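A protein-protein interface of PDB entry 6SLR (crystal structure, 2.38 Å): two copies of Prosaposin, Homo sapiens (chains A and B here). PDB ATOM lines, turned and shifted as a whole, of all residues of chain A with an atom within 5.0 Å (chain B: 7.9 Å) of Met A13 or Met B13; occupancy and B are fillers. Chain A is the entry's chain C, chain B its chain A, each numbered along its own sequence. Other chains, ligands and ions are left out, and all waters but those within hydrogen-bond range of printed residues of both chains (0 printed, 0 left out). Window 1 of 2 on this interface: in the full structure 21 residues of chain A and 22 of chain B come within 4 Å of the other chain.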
ATOM      1  N   VAL A   6      -0.935   5.745 -25.215  1.00  0.00           N
ATOM      2  CA  VAL A   6      -2.392   5.880 -24.904  1.00  0.00           C
ATOM      3  C   VAL A   6      -3.204   5.026 -25.895  1.00  0.00           C
ATOM      4  O   VAL A   6      -4.103   4.305 -25.451  1.00  0.00           O
ATOM      5  CB  VAL A   6      -2.825   7.355 -24.905  1.00  0.00           C
ATOM      6  CG1 VAL A   6      -4.342   7.529 -24.895  1.00  0.00           C
ATOM      7  CG2 VAL A   6      -2.162   8.109 -23.760  1.00  0.00           C
ATOM      8  N   ASP A   9      -2.803   1.321 -24.993  1.00  0.00           N
ATOM      9  CA  ASP A   9      -3.509   1.167 -23.694  1.00  0.00           C
ATOM     10  C   ASP A   9      -5.012   1.062 -23.930  1.00  0.00           C
ATOM     11  O   ASP A   9      -5.648   0.210 -23.310  1.00  0.00           O
ATOM     12  CB  ASP A   9      -3.271   2.350 -22.751  1.00  0.00           C
ATOM     13  CG  ASP A   9      -1.846   2.483 -22.262  1.00  0.00           C
ATOM     14  OD1 ASP A   9      -1.137   1.465 -22.284  1.00  0.00           O
ATOM     15  OD2 ASP A   9      -1.466   3.616 -21.885  1.00  0.00           O
ATOM     16  N   CYS A  10      -5.561   1.945 -24.760  1.00  0.00           N
ATOM     17  CA  CYS A  10      -7.006   1.976 -25.080  1.00  0.00           C
ATOM     18  C   CYS A  10      -7.412   0.653 -25.749  1.00  0.00           C
ATOM     19  O   CYS A  10      -8.417   0.054 -25.309  1.00  0.00           O
ATOM     20  CB  CYS A  10      -7.333   3.168 -25.963  1.00  0.00           C
ATOM     21  SG  CYS A  10      -9.096   3.289 -26.328  1.00  0.00           S
ATOM     22  N   ILE A  11      -6.644   0.186 -26.733  1.00  0.00           N
ATOM     23  CA  ILE A  11      -6.930  -1.102 -27.435  1.00  0.00           C
ATOM     24  C   ILE A  11      -6.945  -2.246 -26.409  1.00  0.00           C
ATOM     25  O   ILE A  11      -7.881  -3.078 -26.451  1.00  0.00           O
ATOM     26  CB  ILE A  11      -5.932  -1.346 -28.583  1.00  0.00           C
ATOM     27  CG1 ILE A  11      -6.160  -0.334 -29.712  1.00  0.00           C
ATOM     28  CG2 ILE A  11      -6.051  -2.777 -29.084  1.00  0.00           C
ATOM     29  CD1 ILE A  11      -5.104  -0.342 -30.791  1.00  0.00           C
ATOM     30  N   GLN A  12      -5.952  -2.294 -25.524  1.00  0.00           N
ATOM     31  CA  GLN A  12      -5.866  -3.331 -24.463  1.00  0.00           C
ATOM     32  C   GLN A  12      -7.130  -3.259 -23.593  1.00  0.00           C
ATOM     33  O   GLN A  12      -7.797  -4.283 -23.441  1.00  0.00           O
ATOM     34  CB  GLN A  12      -4.585  -3.151 -23.636  1.00  0.00           C
ATOM     35  CG  GLN A  12      -4.356  -4.260 -22.616  1.00  0.00           C
ATOM     36  CD  GLN A  12      -4.401  -5.639 -23.238  1.00  0.00           C
ATOM     37  OE1 GLN A  12      -5.388  -6.372 -23.129  1.00  0.00           O
ATOM     38  NE2 GLN A  12      -3.334  -5.994 -23.938  1.00  0.00           N
ATOM     39  N   MET A  13      -7.458  -2.081 -23.056  1.00  0.00           N
ATOM     40  CA  MET A  13      -8.637  -1.870 -22.168  1.00  0.00           C
ATOM     41  C   MET A  13      -9.926  -2.290 -22.886  1.00  0.00           C
ATOM     42  O   MET A  13     -10.733  -3.011 -22.281  1.00  0.00           O
ATOM     43  CB  MET A  13      -8.779  -0.413 -21.722  1.00  0.00           C
ATOM     44  CG  MET A  13      -9.864  -0.222 -20.678  1.00  0.00           C
ATOM     45  SD  MET A  13      -9.915   1.461 -20.044  1.00  0.00           S
ATOM     46  CE  MET A  13     -10.672   2.283 -21.445  1.00  0.00           C
ATOM     47  N   VAL A  14     -10.143  -1.847 -24.118  1.00  0.00           N
ATOM     48  CA  VAL A  14     -11.433  -2.113 -24.814  1.00  0.00           C
ATOM     49  C   VAL A  14     -11.548  -3.615 -25.115  1.00  0.00           C
ATOM     50  O   VAL A  14     -12.645  -4.161 -24.949  1.00  0.00           O
ATOM     51  CB  VAL A  14     -11.591  -1.233 -26.063  1.00  0.00           C
ATOM     52  CG1 VAL A  14     -12.794  -1.660 -26.886  1.00  0.00           C
ATOM     53  CG2 VAL A  14     -11.696   0.234 -25.683  1.00  0.00           C
ATOM     54  N   THR A  15     -10.458  -4.273 -25.504  1.00  0.00           N
ATOM     55  CA  THR A  15     -10.416  -5.744 -25.708  1.00  0.00           C
ATOM     56  C   THR A  15     -10.875  -6.454 -24.423  1.00  0.00           C
ATOM     57  O   THR A  15     -11.712  -7.365 -24.517  1.00  0.00           O
ATOM     58  CB  THR A  15      -9.016  -6.200 -26.126  1.00  0.00           C
ATOM     59  OG1 THR A  15      -8.679  -5.502 -27.321  1.00  0.00           O
ATOM     60  CG2 THR A  15      -8.945  -7.693 -26.353  1.00  0.00           C
ATOM     61  N   ASP A  16     -10.365  -6.037 -23.261  1.00  0.00           N
ATOM     62  CA  ASP A  16     -10.705  -6.650 -21.949  1.00  0.00           C
ATOM     63  C   ASP A  16     -12.167  -6.340 -21.603  1.00  0.00           C
ATOM     64  O   ASP A  16     -12.835  -7.210 -21.028  1.00  0.00           O
ATOM     65  CB  ASP A  16      -9.716  -6.208 -20.862  1.00  0.00           C
ATOM     66  CG  ASP A  16      -8.338  -6.843 -20.997  1.00  0.00           C
ATOM     67  OD1 ASP A  16      -8.251  -7.883 -21.676  1.00  0.00           O
ATOM     68  OD2 ASP A  16      -7.359  -6.283 -20.449  1.00  0.00           O
ATOM     69  N   ILE A  17     -12.665  -5.157 -21.952  1.00  0.00           N
ATOM     70  CA  ILE A  17     -14.095  -4.799 -21.726  1.00  0.00           C
ATOM     71  C   ILE A  17     -14.982  -5.770 -22.512  1.00  0.00           C
ATOM     72  O   ILE A  17     -15.968  -6.273 -21.942  1.00  0.00           O
ATOM     73  CB  ILE A  17     -14.354  -3.331 -22.101  1.00  0.00           C
ATOM     74  CG1 ILE A  17     -13.737  -2.393 -21.057  1.00  0.00           C
ATOM     75  CG2 ILE A  17     -15.841  -3.062 -22.305  1.00  0.00           C
ATOM     76  CD1 ILE A  17     -13.709  -0.944 -21.493  1.00  0.00           C
ATOM     77  N   PHE A  79      -8.481   8.459 -28.882  1.00  0.00           N
ATOM     78  CA  PHE A  79      -7.230   7.960 -28.254  1.00  0.00           C
ATOM     79  C   PHE A  79      -6.325   7.236 -29.266  1.00  0.00           C
ATOM     80  O   PHE A  79      -5.153   6.972 -28.906  1.00  0.00           O
ATOM     81  CB  PHE A  79      -7.534   7.053 -27.062  1.00  0.00           C
ATOM     82  CG  PHE A  79      -8.192   7.742 -25.895  1.00  0.00           C
ATOM     83  CD1 PHE A  79      -7.851   9.035 -25.536  1.00  0.00           C
ATOM     84  CD2 PHE A  79      -9.124   7.073 -25.124  1.00  0.00           C
ATOM     85  CE1 PHE A  79      -8.461   9.655 -24.455  1.00  0.00           C
ATOM     86  CE2 PHE A  79      -9.744   7.699 -24.052  1.00  0.00           C
ATOM     87  CZ  PHE A  79      -9.398   8.983 -23.709  1.00  0.00           C
ATOM     88  N   ASP B   5      -8.871  -6.976 -14.610  1.00  0.00           N
ATOM     89  CA  ASP B   5      -8.087  -6.659 -15.833  1.00  0.00           C
ATOM     90  C   ASP B   5      -8.470  -5.272 -16.336  1.00  0.00           C
ATOM     91  O   ASP B   5      -7.580  -4.490 -16.575  1.00  0.00           O
ATOM     92  CB  ASP B   5      -8.381  -7.616 -16.987  1.00  0.00           C
ATOM     93  CG  ASP B   5      -7.658  -8.939 -16.909  1.00  0.00           C
ATOM     94  OD1 ASP B   5      -6.744  -9.054 -16.074  1.00  0.00           O
ATOM     95  OD2 ASP B   5      -8.017  -9.830 -17.705  1.00  0.00           O
ATOM     96  N   VAL B   6      -9.763  -5.008 -16.502  1.00  0.00           N
ATOM     97  CA  VAL B   6     -10.290  -3.699 -16.984  1.00  0.00           C
ATOM     98  C   VAL B   6      -9.813  -2.591 -16.036  1.00  0.00           C
ATOM     99  O   VAL B   6      -9.325  -1.560 -16.544  1.00  0.00           O
ATOM    100  CB  VAL B   6     -11.824  -3.728 -17.135  1.00  0.00           C
ATOM    101  CG1 VAL B   6     -12.413  -2.336 -17.336  1.00  0.00           C
ATOM    102  CG2 VAL B   6     -12.239  -4.660 -18.263  1.00  0.00           C
ATOM    103  N   CYS B   7      -9.898  -2.800 -14.719  1.00  0.00           N
ATOM    104  CA  CYS B   7      -9.484  -1.779 -13.721  1.00  0.00           C
ATOM    105  C   CYS B   7      -8.010  -1.404 -13.950  1.00  0.00           C
ATOM    106  O   CYS B   7      -7.710  -0.197 -14.114  1.00  0.00           O
ATOM    107  CB  CYS B   7      -9.723  -2.261 -12.299  1.00  0.00           C
ATOM    108  SG  CYS B   7      -9.097  -1.112 -11.049  1.00  0.00           S
ATOM    109  N   GLN B   8      -7.122  -2.394 -14.009  1.00  0.00           N
ATOM    110  CA  GLN B   8      -5.664  -2.164 -14.196  1.00  0.00           C
ATOM    111  C   GLN B   8      -5.390  -1.516 -15.557  1.00  0.00           C
ATOM    112  O   GLN B   8      -4.531  -0.610 -15.612  1.00  0.00           O
ATOM    113  CB  GLN B   8      -4.898  -3.470 -14.002  1.00  0.00           C
ATOM    114  CG  GLN B   8      -4.936  -3.969 -12.562  1.00  0.00           C
ATOM    115  CD  GLN B   8      -4.431  -2.930 -11.588  1.00  0.00           C
ATOM    116  OE1 GLN B   8      -3.533  -2.144 -11.898  1.00  0.00           O
ATOM    117  NE2 GLN B   8      -5.020  -2.906 -10.402  1.00  0.00           N
ATOM    118  N   ASP B   9      -6.072  -1.969 -16.615  1.00  0.00           N
ATOM    119  CA  ASP B   9      -5.975  -1.373 -17.973  1.00  0.00           C
ATOM    120  C   ASP B   9      -6.312   0.115 -17.890  1.00  0.00           C
ATOM    121  O   ASP B   9      -5.609   0.914 -18.509  1.00  0.00           O
ATOM    122  CB  ASP B   9      -6.944  -2.019 -18.969  1.00  0.00           C
ATOM    123  CG  ASP B   9      -6.648  -3.472 -19.308  1.00  0.00           C
ATOM    124  OD1 ASP B   9      -5.495  -3.917 -19.120  1.00  0.00           O
ATOM    125  OD2 ASP B   9      -7.590  -4.164 -19.731  1.00  0.00           O
ATOM    126  N   CYS B  10      -7.388   0.465 -17.193  1.00  0.00           N
ATOM    127  CA  CYS B  10      -7.858   1.859 -17.055  1.00  0.00           C
ATOM    128  C   CYS B  10      -6.784   2.681 -16.323  1.00  0.00           C
ATOM    129  O   CYS B  10      -6.434   3.765 -16.821  1.00  0.00           O
ATOM    130  CB  CYS B  10      -9.202   1.895 -16.335  1.00  0.00           C
ATOM    131  SG  CYS B  10      -9.841   3.574 -16.156  1.00  0.00           S
ATOM    132  N   ILE B  11      -6.236   2.170 -15.219  1.00  0.00           N
ATOM    133  CA  ILE B  11      -5.160   2.857 -14.444  1.00  0.00           C
ATOM    134  C   ILE B  11      -3.958   3.116 -15.364  1.00  0.00           C
ATOM    135  O   ILE B  11      -3.434   4.264 -15.370  1.00  0.00           O
ATOM    136  CB  ILE B  11      -4.786   2.057 -13.184  1.00  0.00           C
ATOM    137  CG1 ILE B  11      -5.929   2.084 -12.164  1.00  0.00           C
ATOM    138  CG2 ILE B  11      -3.481   2.572 -12.577  1.00  0.00           C
ATOM    139  CD1 ILE B  11      -5.745   1.139 -10.991  1.00  0.00           C
ATOM    140  N   GLN B  12      -3.536   2.099 -16.120  1.00  0.00           N
ATOM    141  CA  GLN B  12      -2.394   2.213 -17.065  1.00  0.00           C
ATOM    142  C   GLN B  12      -2.720   3.312 -18.088  1.00  0.00           C
ATOM    143  O   GLN B  12      -1.913   4.229 -18.227  1.00  0.00           O
ATOM    144  CB  GLN B  12      -2.132   0.856 -17.723  1.00  0.00           C
ATOM    145  CG  GLN B  12      -0.928   0.832 -18.653  1.00  0.00           C
ATOM    146  CD  GLN B  12       0.325   1.312 -17.969  1.00  0.00           C
ATOM    147  OE1 GLN B  12       0.684   0.856 -16.889  1.00  0.00           O
ATOM    148  NE2 GLN B  12       0.996   2.266 -18.588  1.00  0.00           N
ATOM    149  N   MET B  13      -3.880   3.238 -18.754  1.00  0.00           N
ATOM    150  CA  MET B  13      -4.302   4.215 -19.798  1.00  0.00           C
ATOM    151  C   MET B  13      -4.335   5.633 -19.218  1.00  0.00           C
ATOM    152  O   MET B  13      -3.790   6.541 -19.860  1.00  0.00           O
ATOM    153  CB  MET B  13      -5.684   3.908 -20.383  1.00  0.00           C
ATOM    154  CG  MET B  13      -5.962   4.749 -21.608  1.00  0.00           C
ATOM    155  SD  MET B  13      -7.485   4.390 -22.469  1.00  0.00           S
ATOM    156  CE  MET B  13      -8.696   4.903 -21.247  1.00  0.00           C
ATOM    157  N   VAL B  14      -4.964   5.840 -18.069  1.00  0.00           N
ATOM    158  CA  VAL B  14      -5.154   7.214 -17.528  1.00  0.00           C
ATOM    159  C   VAL B  14      -3.794   7.790 -17.120  1.00  0.00           C
ATOM    160  O   VAL B  14      -3.566   8.989 -17.397  1.00  0.00           O
ATOM    161  CB  VAL B  14      -6.173   7.237 -16.377  1.00  0.00           C
ATOM    162  CG1 VAL B  14      -6.184   8.585 -15.668  1.00  0.00           C
ATOM    163  CG2 VAL B  14      -7.561   6.871 -16.878  1.00  0.00           C
ATOM    164  N   THR B  15      -2.909   6.976 -16.536  1.00  0.00           N
ATOM    165  CA  THR B  15      -1.520   7.387 -16.203  1.00  0.00           C
ATOM    166  C   THR B  15      -0.828   7.911 -17.465  1.00  0.00           C
ATOM    167  O   THR B  15      -0.200   8.977 -17.412  1.00  0.00           O
ATOM    168  CB  THR B  15      -0.754   6.220 -15.564  1.00  0.00           C
ATOM    169  OG1 THR B  15      -1.444   5.881 -14.356  1.00  0.00           O
ATOM    170  CG2 THR B  15       0.693   6.555 -15.267  1.00  0.00           C
ATOM    171  N   ASP B  16      -0.941   7.182 -18.581  1.00  0.00           N
ATOM    172  CA  ASP B  16      -0.272   7.536 -19.856  1.00  0.00           C
ATOM    173  C   ASP B  16      -0.949   8.785 -20.442  1.00  0.00           C
ATOM    174  O   ASP B  16      -0.257   9.603 -21.058  1.00  0.00           O
ATOM    175  CB  ASP B  16      -0.255   6.329 -20.796  1.00  0.00           C
ATOM    176  CG  ASP B  16       0.747   5.251 -20.379  1.00  0.00           C
ATOM    177  OD1 ASP B  16       1.643   5.550 -19.565  1.00  0.00           O
ATOM    178  OD2 ASP B  16       0.616   4.096 -20.855  1.00  0.00           O
ATOM    179  N   ILE B  17      -2.258   8.955 -20.267  1.00  0.00           N
ATOM    180  CA  ILE B  17      -2.969  10.185 -20.727  1.00  0.00           C
ATOM    181  C   ILE B  17      -2.378  11.398 -20.000  1.00  0.00           C
ATOM    182  O   ILE B  17      -2.103  12.412 -20.661  1.00  0.00           O
ATOM    183  CB  ILE B  17      -4.487  10.047 -20.519  1.00  0.00           C
ATOM    184  CG1 ILE B  17      -5.077   9.076 -21.548  1.00  0.00           C
ATOM    185  CG2 ILE B  17      -5.178  11.404 -20.549  1.00  0.00           C
ATOM    186  CD1 ILE B  17      -6.506   8.682 -21.256  1.00  0.00           C
ATOM    187  N   GLN B  18      -2.191  11.299 -18.690  1.00  0.00           N
ATOM    188  CA  GLN B  18      -1.670  12.423 -17.871  1.00  0.00           C
ATOM    189  C   GLN B  18      -0.245  12.731 -18.345  1.00  0.00           C
ATOM    190  O   GLN B  18       0.059  13.914 -18.564  1.00  0.00           O
ATOM    191  CB  GLN B  18      -1.806  12.103 -16.377  1.00  0.00           C
ATOM    192  CG  GLN B  18      -3.253  12.050 -15.908  1.00  0.00           C
ATOM    193  CD  GLN B  18      -3.381  11.943 -14.405  1.00  0.00           C
ATOM    194  OE1 GLN B  18      -2.531  11.360 -13.724  1.00  0.00           O
ATOM    195  NE2 GLN B  18      -4.482  12.468 -13.883  1.00  0.00           N
ATOM    196  N   THR B  19       0.574  11.706 -18.576  1.00  0.00           N
ATOM    197  CA  THR B  19       1.939  11.863 -19.150  1.00  0.00           C
ATOM    198  C   THR B  19       1.834  12.628 -20.477  1.00  0.00           C
ATOM    199  O   THR B  19       2.584  13.615 -20.660  1.00  0.00           O
ATOM    200  CB  THR B  19       2.623  10.497 -19.278  1.00  0.00           C
ATOM    201  OG1 THR B  19       2.748   9.967 -17.959  1.00  0.00           O
ATOM    202  CG2 THR B  19       3.973  10.545 -19.955  1.00  0.00           C
ATOM    203  N   ALA B  20       0.896  12.226 -21.340  1.00  0.00           N
ATOM    204  CA  ALA B  20       0.690  12.823 -22.681  1.00  0.00           C
ATOM    205  C   ALA B  20       0.364  14.306 -22.522  1.00  0.00           C
ATOM    206  O   ALA B  20       0.986  15.148 -23.210  1.00  0.00           O
ATOM    207  CB  ALA B  20      -0.413  12.115 -23.430  1.00  0.00           C
ATOM    208  N   PHE B  27      -1.819  17.550 -27.559  1.00  0.00           N
ATOM    209  CA  PHE B  27      -2.630  16.350 -27.231  1.00  0.00           C
ATOM    210  C   PHE B  27      -4.072  16.745 -26.877  1.00  0.00           C
ATOM    211  O   PHE B  27      -4.997  16.287 -27.565  1.00  0.00           O
ATOM    212  CB  PHE B  27      -1.963  15.558 -26.102  1.00  0.00           C
ATOM    213  CG  PHE B  27      -2.704  14.301 -25.737  1.00  0.00           C
ATOM    214  CD1 PHE B  27      -2.555  13.142 -26.488  1.00  0.00           C
ATOM    215  CD2 PHE B  27      -3.583  14.282 -24.667  1.00  0.00           C
ATOM    216  CE1 PHE B  27      -3.257  11.994 -26.167  1.00  0.00           C
ATOM    217  CE2 PHE B  27      -4.286  13.130 -24.349  1.00  0.00           C
ATOM    218  CZ  PHE B  27      -4.129  11.994 -25.099  1.00  0.00           C
ATOM    219  N   PRO B  70      -5.102   8.469 -11.180  1.00  0.00           N
ATOM    220  CA  PRO B  70      -5.681   7.527 -12.140  1.00  0.00           C
ATOM    221  C   PRO B  70      -6.747   6.602 -11.530  1.00  0.00           C
ATOM    222  O   PRO B  70      -7.771   6.431 -12.153  1.00  0.00           O
ATOM    223  CB  PRO B  70      -4.444   6.763 -12.623  1.00  0.00           C
ATOM    224  CG  PRO B  70      -3.353   7.821 -12.571  1.00  0.00           C
ATOM    225  CD  PRO B  70      -3.636   8.565 -11.280  1.00  0.00           C
ATOM    226  N   ILE B  73     -10.041   8.431 -11.084  1.00  0.00           N
ATOM    227  CA  ILE B  73     -10.713   8.652 -12.396  1.00  0.00           C
ATOM    228  C   ILE B  73     -11.404   7.346 -12.812  1.00  0.00           C
ATOM    229  O   ILE B  73     -12.594   7.385 -13.183  1.00  0.00           O
ATOM    230  CB  ILE B  73      -9.696   9.154 -13.438  1.00  0.00           C
ATOM    231  CG1 ILE B  73      -9.176  10.547 -13.073  1.00  0.00           C
ATOM    232  CG2 ILE B  73     -10.289   9.127 -14.839  1.00  0.00           C
ATOM    233  CD1 ILE B  73      -7.858  10.914 -13.734  1.00  0.00           C
ATOM    234  N   CYS B  74     -10.699   6.226 -12.702  1.00  0.00           N
ATOM    235  CA  CYS B  74     -11.192   4.885 -13.114  1.00  0.00           C
ATOM    236  C   CYS B  74     -12.370   4.453 -12.234  1.00  0.00           C
ATOM    237  O   CYS B  74     -13.386   3.969 -12.795  1.00  0.00           O
ATOM    238  CB  CYS B  74     -10.052   3.881 -13.104  1.00  0.00           C
ATOM    239  SG  CYS B  74      -8.876   4.246 -14.432  1.00  0.00           S
ATOM    240  N   VAL B  77     -15.446   6.602 -13.298  1.00  0.00           N
ATOM    241  CA  VAL B  77     -16.106   6.105 -14.539  1.00  0.00           C
ATOM    242  C   VAL B  77     -16.733   4.730 -14.287  1.00  0.00           C
ATOM    243  O   VAL B  77     -17.652   4.374 -15.042  1.00  0.00           O
ATOM    244  CB  VAL B  77     -15.118   6.086 -15.716  1.00  0.00           C
ATOM    245  CG1 VAL B  77     -15.720   5.446 -16.954  1.00  0.00           C
ATOM    246  CG2 VAL B  77     -14.638   7.494 -16.029  1.00  0.00           C
ATOM    247  N   PHE B  79     -14.905   1.653 -13.900  1.00  0.00           N
ATOM    248  CA  PHE B  79     -14.021   0.539 -14.334  1.00  0.00           C
ATOM    249  C   PHE B  79     -13.191  -0.018 -13.164  1.00  0.00           C
ATOM    250  O   PHE B  79     -12.565  -1.085 -13.360  1.00  0.00           O
ATOM    251  CB  PHE B  79     -13.102   0.986 -15.474  1.00  0.00           C
ATOM    252  CG  PHE B  79     -13.811   1.334 -16.758  1.00  0.00           C
ATOM    253  CD1 PHE B  79     -14.926   0.620 -17.181  1.00  0.00           C
ATOM    254  CD2 PHE B  79     -13.334   2.353 -17.567  1.00  0.00           C
ATOM    255  CE1 PHE B  79     -15.556   0.937 -18.373  1.00  0.00           C
ATOM    256  CE2 PHE B  79     -13.974   2.678 -18.752  1.00  0.00           C
ATOM    257  CZ  PHE B  79     -15.083   1.965 -19.154  1.00  0.00           C
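OD2 of Asp A16 sits close to OD2 of Asp B9 (2.2 Å). The side-chain carboxylate (OD2) of Asp A9 sits close to the side-chain carboxylate (OD2) of Asp B16, at 2.4 Å.
Among the printed residues, merely in contact across the chains: Val A6 with Asp B16 (3.6 Å), Val A6 with Ile B17 (3.6 Å), Asp A9 with Gln B12 (3.7 Å), Asp A9 with Met B13 (3.6 Å), Cys A10 with Met B13 (3.6 Å), Gln A12 with Asp B9 (3.7 Å), Met A13 with Asp B9 (3.5 Å), Met A13 with Cys B10 (3.7 Å), Met A13 with Met B13 (3.3 Å), Asp A16 with Asp B5 (3.8 Å), Asp A16 with Val B6 (3.7 Å), Ile A17 with Val B6 (3.7 Å), Ile A17 with Phe B79 (3.98 Å) and Phe A79 with Ile B17 (3.8 Å).
Printed residues of chain B within 4 Å of Val A6: Asp B16 and Ile B17. Of the printed residues of chain B, Asp A9 touches Gln B12, Met B13 and Asp B16. Of the printed residues of chain B, Met A13 touches Asp B9, Cys B10 and Met B13. Of chain A, only Asp A9, Cys A10 and Met A13 come within 4 Å of Met B13. Of the printed residues of chain A, Asp B16 touches Val A6 (3.6 Å) and Asp A9 (2.4 Å). Of the printed residues of chain A, Ile B17 touches Val A6 (3.6 Å) and Phe A79 (3.8 Å). Printed residues of chain A within 4 Å of Phe B79: Ile A17 (3.98 Å). The nearest residue of chain B that does not touch Met A13 is Phe B79 (4.3 Å). The nearest residue of chain A that does not touch Met B13 is Phe A79 (4.1 Å). The nearest printed residue of chain B that does not touch Ile A17 is Asp B9 (5.6 Å).
The backbone carbonyl oxygen (O) of Phe B79 lies close to the backbone NH (N) of Cys B7, at 3.4 Å. N of Phe B79 is in hydrogen-bond range of O of Cys B74 (3.0 Å). OE1 of Gln A12 sits close to OD2 of Asp A16 (3.3 Å). The side-chain amide nitrogen of Gln B12 sits at hydrogen-bond distance from the side-chain carboxylate of Asp B16 (2.9 Å). SG of Cys B74 is disulfide-bonded to SG of Cys B10, at 2.1 Å.
Asp A9 touches Met B13, and with the chains exchanged Met A13 touches Asp B9. Asp A9 touches Asp B16, and with the chains exchanged Asp A16 touches Asp B9. Met A13 touches its own counterpart, Met B13. Ile A17 touches Phe B79, and with the chains exchanged Phe A79 touches Ile B17.
Hydrophobic or aromatic side chains of chain A that line the printed part of chain B: Val A6, Met A13, Ile A17 and Phe A79. Hydrophobic or aromatic side chains of chain B that line the printed part of chain A: Val B6, Met B13, Ile B17 and Phe B79. Along chain B the printed residues that touch a printed residue of chain A span positions 5 to 79. Among the printed residues, no Asp or Glu carboxylate lies within 4 Å of a Lys or Arg side-chain nitrogen of the other chain.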
